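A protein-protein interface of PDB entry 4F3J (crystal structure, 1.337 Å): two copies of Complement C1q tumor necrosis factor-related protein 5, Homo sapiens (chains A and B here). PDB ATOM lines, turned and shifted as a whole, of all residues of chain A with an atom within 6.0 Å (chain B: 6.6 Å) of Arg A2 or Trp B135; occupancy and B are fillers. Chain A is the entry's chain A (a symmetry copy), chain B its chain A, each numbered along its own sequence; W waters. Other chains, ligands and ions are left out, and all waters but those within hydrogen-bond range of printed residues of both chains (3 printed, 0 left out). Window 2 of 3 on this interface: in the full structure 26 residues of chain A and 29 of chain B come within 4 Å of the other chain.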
ATOM      1  N   ALA A   1      16.441   7.847   6.562  1.00  0.00           N
ATOM      2  CA  ALA A   1      16.641   6.503   5.999  1.00  0.00           C
ATOM      3  C   ALA A   1      17.800   6.470   5.026  1.00  0.00           C
ATOM      4  O   ALA A   1      18.177   7.508   4.467  1.00  0.00           O
ATOM      5  CB  ALA A   1      15.375   6.013   5.329  1.00  0.00           C
ATOM      6  N   ARG A   2      18.350   5.275   4.796  1.00  0.00           N
ATOM      7  CA  ARG A   2      19.511   5.107   3.925  1.00  0.00           C
ATOM      8  C   ARG A   2      19.215   4.074   2.853  1.00  0.00           C
ATOM      9  O   ARG A   2      18.813   2.949   3.151  1.00  0.00           O
ATOM     10  CB  ARG A   2      20.708   4.643   4.763  1.00  0.00           C
ATOM     11  CG  ARG A   2      21.109   5.622   5.854  1.00  0.00           C
ATOM     12  CD  ARG A   2      22.228   5.017   6.673  1.00  0.00           C
ATOM     13  NE  ARG A   2      22.878   6.000   7.534  1.00  0.00           N
ATOM     14  CZ  ARG A   2      22.440   6.321   8.745  1.00  0.00           C
ATOM     15  NH1 ARG A   2      21.353   5.734   9.236  1.00  0.00           N
ATOM     16  NH2 ARG A   2      23.088   7.224   9.465  1.00  0.00           N
ATOM     17  N   SER A   3      19.407   4.457   1.600  1.00  0.00           N
ATOM     18  CA  SER A   3      19.399   3.494   0.514  1.00  0.00           C
ATOM     19  C   SER A   3      20.127   4.103  -0.664  1.00  0.00           C
ATOM     20  O   SER A   3      19.708   5.137  -1.193  1.00  0.00           O
ATOM     21  CB  SER A   3      17.972   3.128   0.116  1.00  0.00           C
ATOM     22  OG  SER A   3      18.008   2.186  -0.952  1.00  0.00           O
ATOM     23  N   ALA A   4      21.223   3.473  -1.083  1.00  0.00           N
ATOM     24  CA  ALA A   4      21.973   3.961  -2.224  1.00  0.00           C
ATOM     25  C   ALA A   4      22.809   2.863  -2.826  1.00  0.00           C
ATOM     26  O   ALA A   4      23.249   1.949  -2.113  1.00  0.00           O
ATOM     27  CB  ALA A   4      22.902   5.114  -1.811  1.00  0.00           C
ATOM     28  N   GLN A  32      23.519  -1.306   1.759  1.00  0.00           N
ATOM     29  CA  GLN A  32      22.293  -1.973   2.212  1.00  0.00           C
ATOM     30  C   GLN A  32      22.031  -3.288   1.478  1.00  0.00           C
ATOM     31  O   GLN A  32      21.152  -4.055   1.872  1.00  0.00           O
ATOM     32  CB  GLN A  32      21.074  -1.051   2.026  1.00  0.00           C
ATOM     33  CG  GLN A  32      21.111   0.265   2.813  1.00  0.00           C
ATOM     34  CD  GLN A  32      22.103   1.275   2.251  1.00  0.00           C
ATOM     35  OE1 GLN A  32      22.162   1.505   1.043  1.00  0.00           O
ATOM     36  NE2 GLN A  32      22.862   1.907   3.134  1.00  0.00           N
ATOM     37  N   HIS A  34      20.687  -3.371  -1.365  1.00  0.00           N
ATOM     38  CA  HIS A  34      19.438  -3.181  -2.101  1.00  0.00           C
ATOM     39  C   HIS A  34      19.607  -3.404  -3.614  1.00  0.00           C
ATOM     40  O   HIS A  34      18.638  -3.739  -4.306  1.00  0.00           O
ATOM     41  CB  HIS A  34      18.852  -1.801  -1.820  1.00  0.00           C
ATOM     42  CG  HIS A  34      18.386  -1.630  -0.410  1.00  0.00           C
ATOM     43  ND1 HIS A  34      18.068  -0.395   0.125  1.00  0.00           N
ATOM     44  CD2 HIS A  34      18.170  -2.530   0.575  1.00  0.00           C
ATOM     45  CE1 HIS A  34      17.690  -0.547   1.380  1.00  0.00           C
ATOM     46  NE2 HIS A  34      17.735  -1.834   1.677  1.00  0.00           N
ATOM     47  N   VAL A  46      12.728   0.689   1.478  1.00  0.00           N
ATOM     48  CA  VAL A  46      12.244   1.867   2.187  1.00  0.00           C
ATOM     49  C   VAL A  46      11.343   2.630   1.237  1.00  0.00           C
ATOM     50  O   VAL A  46      11.801   3.066   0.181  1.00  0.00           O
ATOM     51  CB  VAL A  46      13.406   2.802   2.606  1.00  0.00           C
ATOM     52  CG1 VAL A  46      12.872   4.057   3.297  1.00  0.00           C
ATOM     53  CG2 VAL A  46      14.423   2.059   3.462  1.00  0.00           C
ATOM     54  N   LEU A 130      17.799   6.905  -2.413  1.00  0.00           N
ATOM     55  CA  LEU A 130      16.660   7.483  -1.738  1.00  0.00           C
ATOM     56  C   LEU A 130      16.951   8.941  -1.427  1.00  0.00           C
ATOM     57  O   LEU A 130      17.979   9.272  -0.793  1.00  0.00           O
ATOM     58  CB  LEU A 130      16.359   6.712  -0.443  1.00  0.00           C
ATOM     59  CG  LEU A 130      15.258   7.231   0.465  1.00  0.00           C
ATOM     60  CD1 LEU A 130      13.915   6.836  -0.071  1.00  0.00           C
ATOM     61  CD2 LEU A 130      15.395   6.584   1.830  1.00  0.00           C
ATOM     62  N   ALA B   1      23.208  15.341   8.203  1.00  0.00           N
ATOM     63  CA  ALA B   1      24.458  16.045   7.881  1.00  0.00           C
ATOM     64  C   ALA B   1      24.359  16.795   6.570  1.00  0.00           C
ATOM     65  O   ALA B   1      23.526  16.455   5.719  1.00  0.00           O
ATOM     66  CB  ALA B   1      25.620  15.075   7.848  1.00  0.00           C
ATOM     67  N   GLN B  45      34.551  15.770   4.945  1.00  0.00           N
ATOM     68  CA  GLN B  45      34.578  15.954   6.404  1.00  0.00           C
ATOM     69  C   GLN B  45      33.530  15.111   7.127  1.00  0.00           C
ATOM     70  O   GLN B  45      33.605  14.921   8.319  1.00  0.00           O
ATOM     71  CB  GLN B  45      34.392  17.433   6.759  1.00  0.00           C
ATOM     72  CG  GLN B  45      35.408  18.367   6.087  1.00  0.00           C
ATOM     73  CD  GLN B  45      36.846  18.101   6.530  1.00  0.00           C
ATOM     74  OE1 GLN B  45      37.082  17.543   7.603  1.00  0.00           O
ATOM     75  NE2 GLN B  45      37.810  18.494   5.693  1.00  0.00           N
ATOM     76  N   VAL B  46      32.542  14.612   6.404  1.00  0.00           N
ATOM     77  CA  VAL B  46      31.493  13.789   6.997  1.00  0.00           C
ATOM     78  C   VAL B  46      31.550  12.432   6.328  1.00  0.00           C
ATOM     79  O   VAL B  46      31.367  12.344   5.113  1.00  0.00           O
ATOM     80  CB  VAL B  46      30.087  14.390   6.756  1.00  0.00           C
ATOM     81  CG1 VAL B  46      29.001  13.484   7.336  1.00  0.00           C
ATOM     82  CG2 VAL B  46      30.000  15.812   7.292  1.00  0.00           C
ATOM     83  N   PRO B  47      31.824  11.359   7.085  1.00  0.00           N
ATOM     84  CA  PRO B  47      31.841  10.058   6.398  1.00  0.00           C
ATOM     85  C   PRO B  47      30.464   9.688   5.849  1.00  0.00           C
ATOM     86  O   PRO B  47      29.440   9.956   6.488  1.00  0.00           O
ATOM     87  CB  PRO B  47      32.227   9.084   7.516  1.00  0.00           C
ATOM     88  CG  PRO B  47      31.710   9.751   8.786  1.00  0.00           C
ATOM     89  CD  PRO B  47      31.921  11.224   8.551  1.00  0.00           C
ATOM     90  N   GLY B  48      30.419   9.088   4.667  1.00  0.00           N
ATOM     91  CA  GLY B  48      29.117   8.754   4.120  1.00  0.00           C
ATOM     92  C   GLY B  48      29.200   8.409   2.670  1.00  0.00           C
ATOM     93  O   GLY B  48      30.284   8.229   2.121  1.00  0.00           O
ATOM     94  N   PRO B 100      36.509  11.007   6.266  1.00  0.00           N
ATOM     95  CA  PRO B 100      37.105  12.346   6.368  1.00  0.00           C
ATOM     96  C   PRO B 100      38.541  12.396   5.841  1.00  0.00           C
ATOM     97  O   PRO B 100      39.329  11.476   6.071  1.00  0.00           O
ATOM     98  CB  PRO B 100      37.029  12.644   7.869  1.00  0.00           C
ATOM     99  CG  PRO B 100      35.751  11.956   8.266  1.00  0.00           C
ATOM    100  CD  PRO B 100      35.809  10.639   7.512  1.00  0.00           C
ATOM    101  N   TYR B 132      23.794  10.220   2.331  1.00  0.00           N
ATOM    102  CA  TYR B 132      23.547   9.866   3.716  1.00  0.00           C
ATOM    103  C   TYR B 132      24.873   9.755   4.448  1.00  0.00           C
ATOM    104  O   TYR B 132      25.925   9.468   3.858  1.00  0.00           O
ATOM    105  CB  TYR B 132      22.703   8.581   3.887  1.00  0.00           C
ATOM    106  CG  TYR B 132      23.331   7.282   3.408  1.00  0.00           C
ATOM    107  CD1 TYR B 132      24.359   6.671   4.133  1.00  0.00           C
ATOM    108  CD2 TYR B 132      22.869   6.634   2.258  1.00  0.00           C
ATOM    109  CE1 TYR B 132      24.931   5.484   3.716  1.00  0.00           C
ATOM    110  CE2 TYR B 132      23.435   5.415   1.845  1.00  0.00           C
ATOM    111  CZ  TYR B 132      24.473   4.863   2.584  1.00  0.00           C
ATOM    112  OH  TYR B 132      25.055   3.662   2.202  1.00  0.00           O
ATOM    113  N   SER B 133      24.795   9.984   5.748  1.00  0.00           N
ATOM    114  CA  SER B 133      25.952   9.959   6.604  1.00  0.00           C
ATOM    115  C   SER B 133      26.202   8.556   7.141  1.00  0.00           C
ATOM    116  O   SER B 133      25.259   7.799   7.419  1.00  0.00           O
ATOM    117  CB  SER B 133      25.732  10.928   7.758  1.00  0.00           C
ATOM    118  OG  SER B 133      26.553  10.592   8.828  1.00  0.00           O
ATOM    119  N   ASP B 134      27.469   8.192   7.291  1.00  0.00           N
ATOM    120  CA  ASP B 134      27.757   6.900   7.913  1.00  0.00           C
ATOM    121  C   ASP B 134      28.090   6.994   9.395  1.00  0.00           C
ATOM    122  O   ASP B 134      28.690   6.087   9.975  1.00  0.00           O
ATOM    123  CB  ASP B 134      28.805   6.120   7.112  1.00  0.00           C
ATOM    124  CG  ASP B 134      28.170   5.226   6.046  1.00  0.00           C
ATOM    125  OD1 ASP B 134      27.030   4.747   6.261  1.00  0.00           O
ATOM    126  OD2 ASP B 134      28.808   4.994   5.008  1.00  0.00           O
ATOM    127  N   TRP B 135      27.692   8.110  10.002  1.00  0.00           N
ATOM    128  CA  TRP B 135      27.596   8.184  11.449  1.00  0.00           C
ATOM    129  C   TRP B 135      26.184   7.738  11.810  1.00  0.00           C
ATOM    130  O   TRP B 135      25.254   8.555  11.855  1.00  0.00           O
ATOM    131  CB  TRP B 135      27.866   9.611  11.965  1.00  0.00           C
ATOM    132  CG  TRP B 135      29.338   9.996  11.993  1.00  0.00           C
ATOM    133  CD1 TRP B 135      30.392   9.182  12.289  1.00  0.00           C
ATOM    134  CD2 TRP B 135      29.899  11.299  11.732  1.00  0.00           C
ATOM    135  NE1 TRP B 135      31.572   9.889  12.225  1.00  0.00           N
ATOM    136  CE2 TRP B 135      31.298  11.191  11.886  1.00  0.00           C
ATOM    137  CE3 TRP B 135      29.355  12.538  11.364  1.00  0.00           C
ATOM    138  CZ2 TRP B 135      32.166  12.275  11.689  1.00  0.00           C
ATOM    139  CZ3 TRP B 135      30.222  13.627  11.182  1.00  0.00           C
ATOM    140  CH2 TRP B 135      31.607  13.482  11.339  1.00  0.00           C
ATOM    141  N   HIS B 136      26.027   6.436  12.047  1.00  0.00           N
ATOM    142  CA  HIS B 136      24.744   5.849  12.437  1.00  0.00           C
ATOM    143  C   HIS B 136      24.326   6.197  13.881  1.00  0.00           C
ATOM    144  O   HIS B 136      25.166   6.540  14.726  1.00  0.00           O
ATOM    145  CB  HIS B 136      24.791   4.324  12.257  1.00  0.00           C
ATOM    146  CG  HIS B 136      25.135   3.889  10.864  1.00  0.00           C
ATOM    147  ND1 HIS B 136      26.433   3.695  10.443  1.00  0.00           N
ATOM    148  CD2 HIS B 136      24.348   3.613   9.798  1.00  0.00           C
ATOM    149  CE1 HIS B 136      26.431   3.314   9.178  1.00  0.00           C
ATOM    150  NE2 HIS B 136      25.178   3.258   8.763  1.00  0.00           N
ATOM    151  N   SER B 137      23.029   6.061  14.161  1.00  0.00           N
ATOM    152  CA  SER B 137      22.443   6.402  15.469  1.00  0.00           C
ATOM    153  C   SER B 137      22.761   5.437  16.613  1.00  0.00           C
ATOM    154  O   SER B 137      22.801   5.835  17.774  1.00  0.00           O
ATOM    155  CB  SER B 137      20.923   6.548  15.358  1.00  0.00           C
ATOM    156  OG  SER B 137      20.573   7.815  14.829  1.00  0.00           O
ATOM    157  N   SER B 138      22.962   4.166  16.285  1.00  0.00           N
ATOM    158  CA  SER B 138      23.362   3.170  17.277  1.00  0.00           C
ATOM    159  C   SER B 138      24.694   2.574  16.845  1.00  0.00           C
ATOM    160  O   SER B 138      24.754   1.394  16.489  1.00  0.00           O
ATOM    161  CB  SER B 138      22.314   2.057  17.359  1.00  0.00           C
ATOM    162  OG  SER B 138      21.031   2.575  17.675  1.00  0.00           O
ATOM    163  N   PRO B 139      25.769   3.385  16.877  1.00  0.00           N
ATOM    164  CA  PRO B 139      27.005   3.009  16.179  1.00  0.00           C
ATOM    165  C   PRO B 139      27.717   1.815  16.796  1.00  0.00           C
ATOM    166  O   PRO B 139      28.474   1.126  16.104  1.00  0.00           O
ATOM    167  CB  PRO B 139      27.875   4.269  16.319  1.00  0.00           C
ATOM    168  CG  PRO B 139      27.344   4.951  17.527  1.00  0.00           C
ATOM    169  CD  PRO B 139      25.877   4.725  17.473  1.00  0.00           C
ATOM    170  N   HIS B 143      25.736  -2.359  13.342  1.00  0.00           N
ATOM    171  CA  HIS B 143      26.690  -1.914  12.319  1.00  0.00           C
ATOM    172  C   HIS B 143      28.108  -2.424  12.563  1.00  0.00           C
ATOM    173  O   HIS B 143      28.516  -3.436  11.997  1.00  0.00           O
ATOM    174  CB  HIS B 143      26.686  -0.380  12.215  1.00  0.00           C
ATOM    175  CG  HIS B 143      25.325   0.232  12.366  1.00  0.00           C
ATOM    176  ND1 HIS B 143      24.381   0.213  11.359  1.00  0.00           N
ATOM    177  CD2 HIS B 143      24.749   0.876  13.409  1.00  0.00           C
ATOM    178  CE1 HIS B 143      23.284   0.821  11.776  1.00  0.00           C
ATOM    179  NE2 HIS B 143      23.480   1.232  13.017  1.00  0.00           N
HETATM  180  O   HOH W   1      20.956   5.450  12.305  1.00  0.00           O
HETATM  181  O   HOH W   2      25.314   2.365  -0.276  1.00  0.00           O
HETATM  182  O   HOH W   3      21.191   8.091  11.866  1.00  0.00           O
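NH2 of Arg A2 sits at hydrogen-bond distance from O of Trp B135, at 3.5 Å.
The guanidinium group of Arg A2 lies within hydrogen-bond range of the backbone carbonyl oxygen of Ser B133 (3.0 Å).
NE2 of Gln A32 lies within hydrogen-bond range of OH of Tyr B132.
The side-chain amide oxygen (OE1) of Gln A32 lies within hydrogen-bond range of the backbone NH (N) of Ala A4.
O of Asp B134 sits at hydrogen-bond distance from ND1 of His B136, at 3.3 Å.
N of Trp B135 lies within hydrogen-bond range of OG of Ser B133, at 3.0 Å.
Tyr B132 touches Arg A2 (CG to CG, 3.7 Å).
CD2 of His B136 touches CZ of Arg A2, 3.5 Å away.
CB of Ala A4 touches CE2 of Tyr B132, 3.7 Å away.
Of chain B, only Tyr B132 (3.7 Å), Ser B133 (3.0 Å), Trp B135 (3.5 Å) and His B136 (3.5 Å) come within 4 Å of Arg A2.
Of the printed residues of chain B, Ala A4 touches Tyr B132.
Of the printed residues of chain B, Gln A32 touches Tyr B132.
Of the printed residues of chain A, Tyr B132 touches Arg A2, Ala A4 and Gln A32.
Of the printed residues of chain A, Ser B133 touches Arg A2 (3.0 Å).
Of the printed residues of chain A, His B136 touches Arg A2 (3.5 Å).
Ser B137 touches none of the printed residues of chain A.
The nearest printed residue of chain A that does not touch His B136 is Gln A32 (6.2 Å).
Of the 8 printed residues of chain A, 3 touch a printed residue of chain B.
Hydrophobic or aromatic side chains of chain A within 4 Å of the printed part of chain B: Ala A4.
Along chain A the printed residues that touch a printed residue of chain B span positions 2 to 32.
Of the 15 printed residues of chain B, 4 touch a printed residue of chain A.
Printed residues of chain B that touch a printed residue of chain A: Tyr B132, Ser B133, Trp B135 and His B136.
Hydrophobic or aromatic side chains of chain B that line the printed part of chain A: Tyr B132 and His B136.
Along chain B the printed residues that touch a printed residue of chain A span positions 132 to 136.
Among the printed residues, 6 pairs touch across the chains.
2 positions are printed for both chains.
Water W2 lies within hydrogen-bond range of the backbone carbonyl oxygen of Ala A4 (2.8 Å) and the side-chain hydroxyl of Tyr B132 (2.8 Å).
Water W1 lies within hydrogen-bond range of the backbone NH of Ser B137 and the guanidinium group of Arg A2.
Water W3 lies within hydrogen-bond range of OG of Ser B137 (3.0 Å) and NH2 of Arg A2 (3.2 Å).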
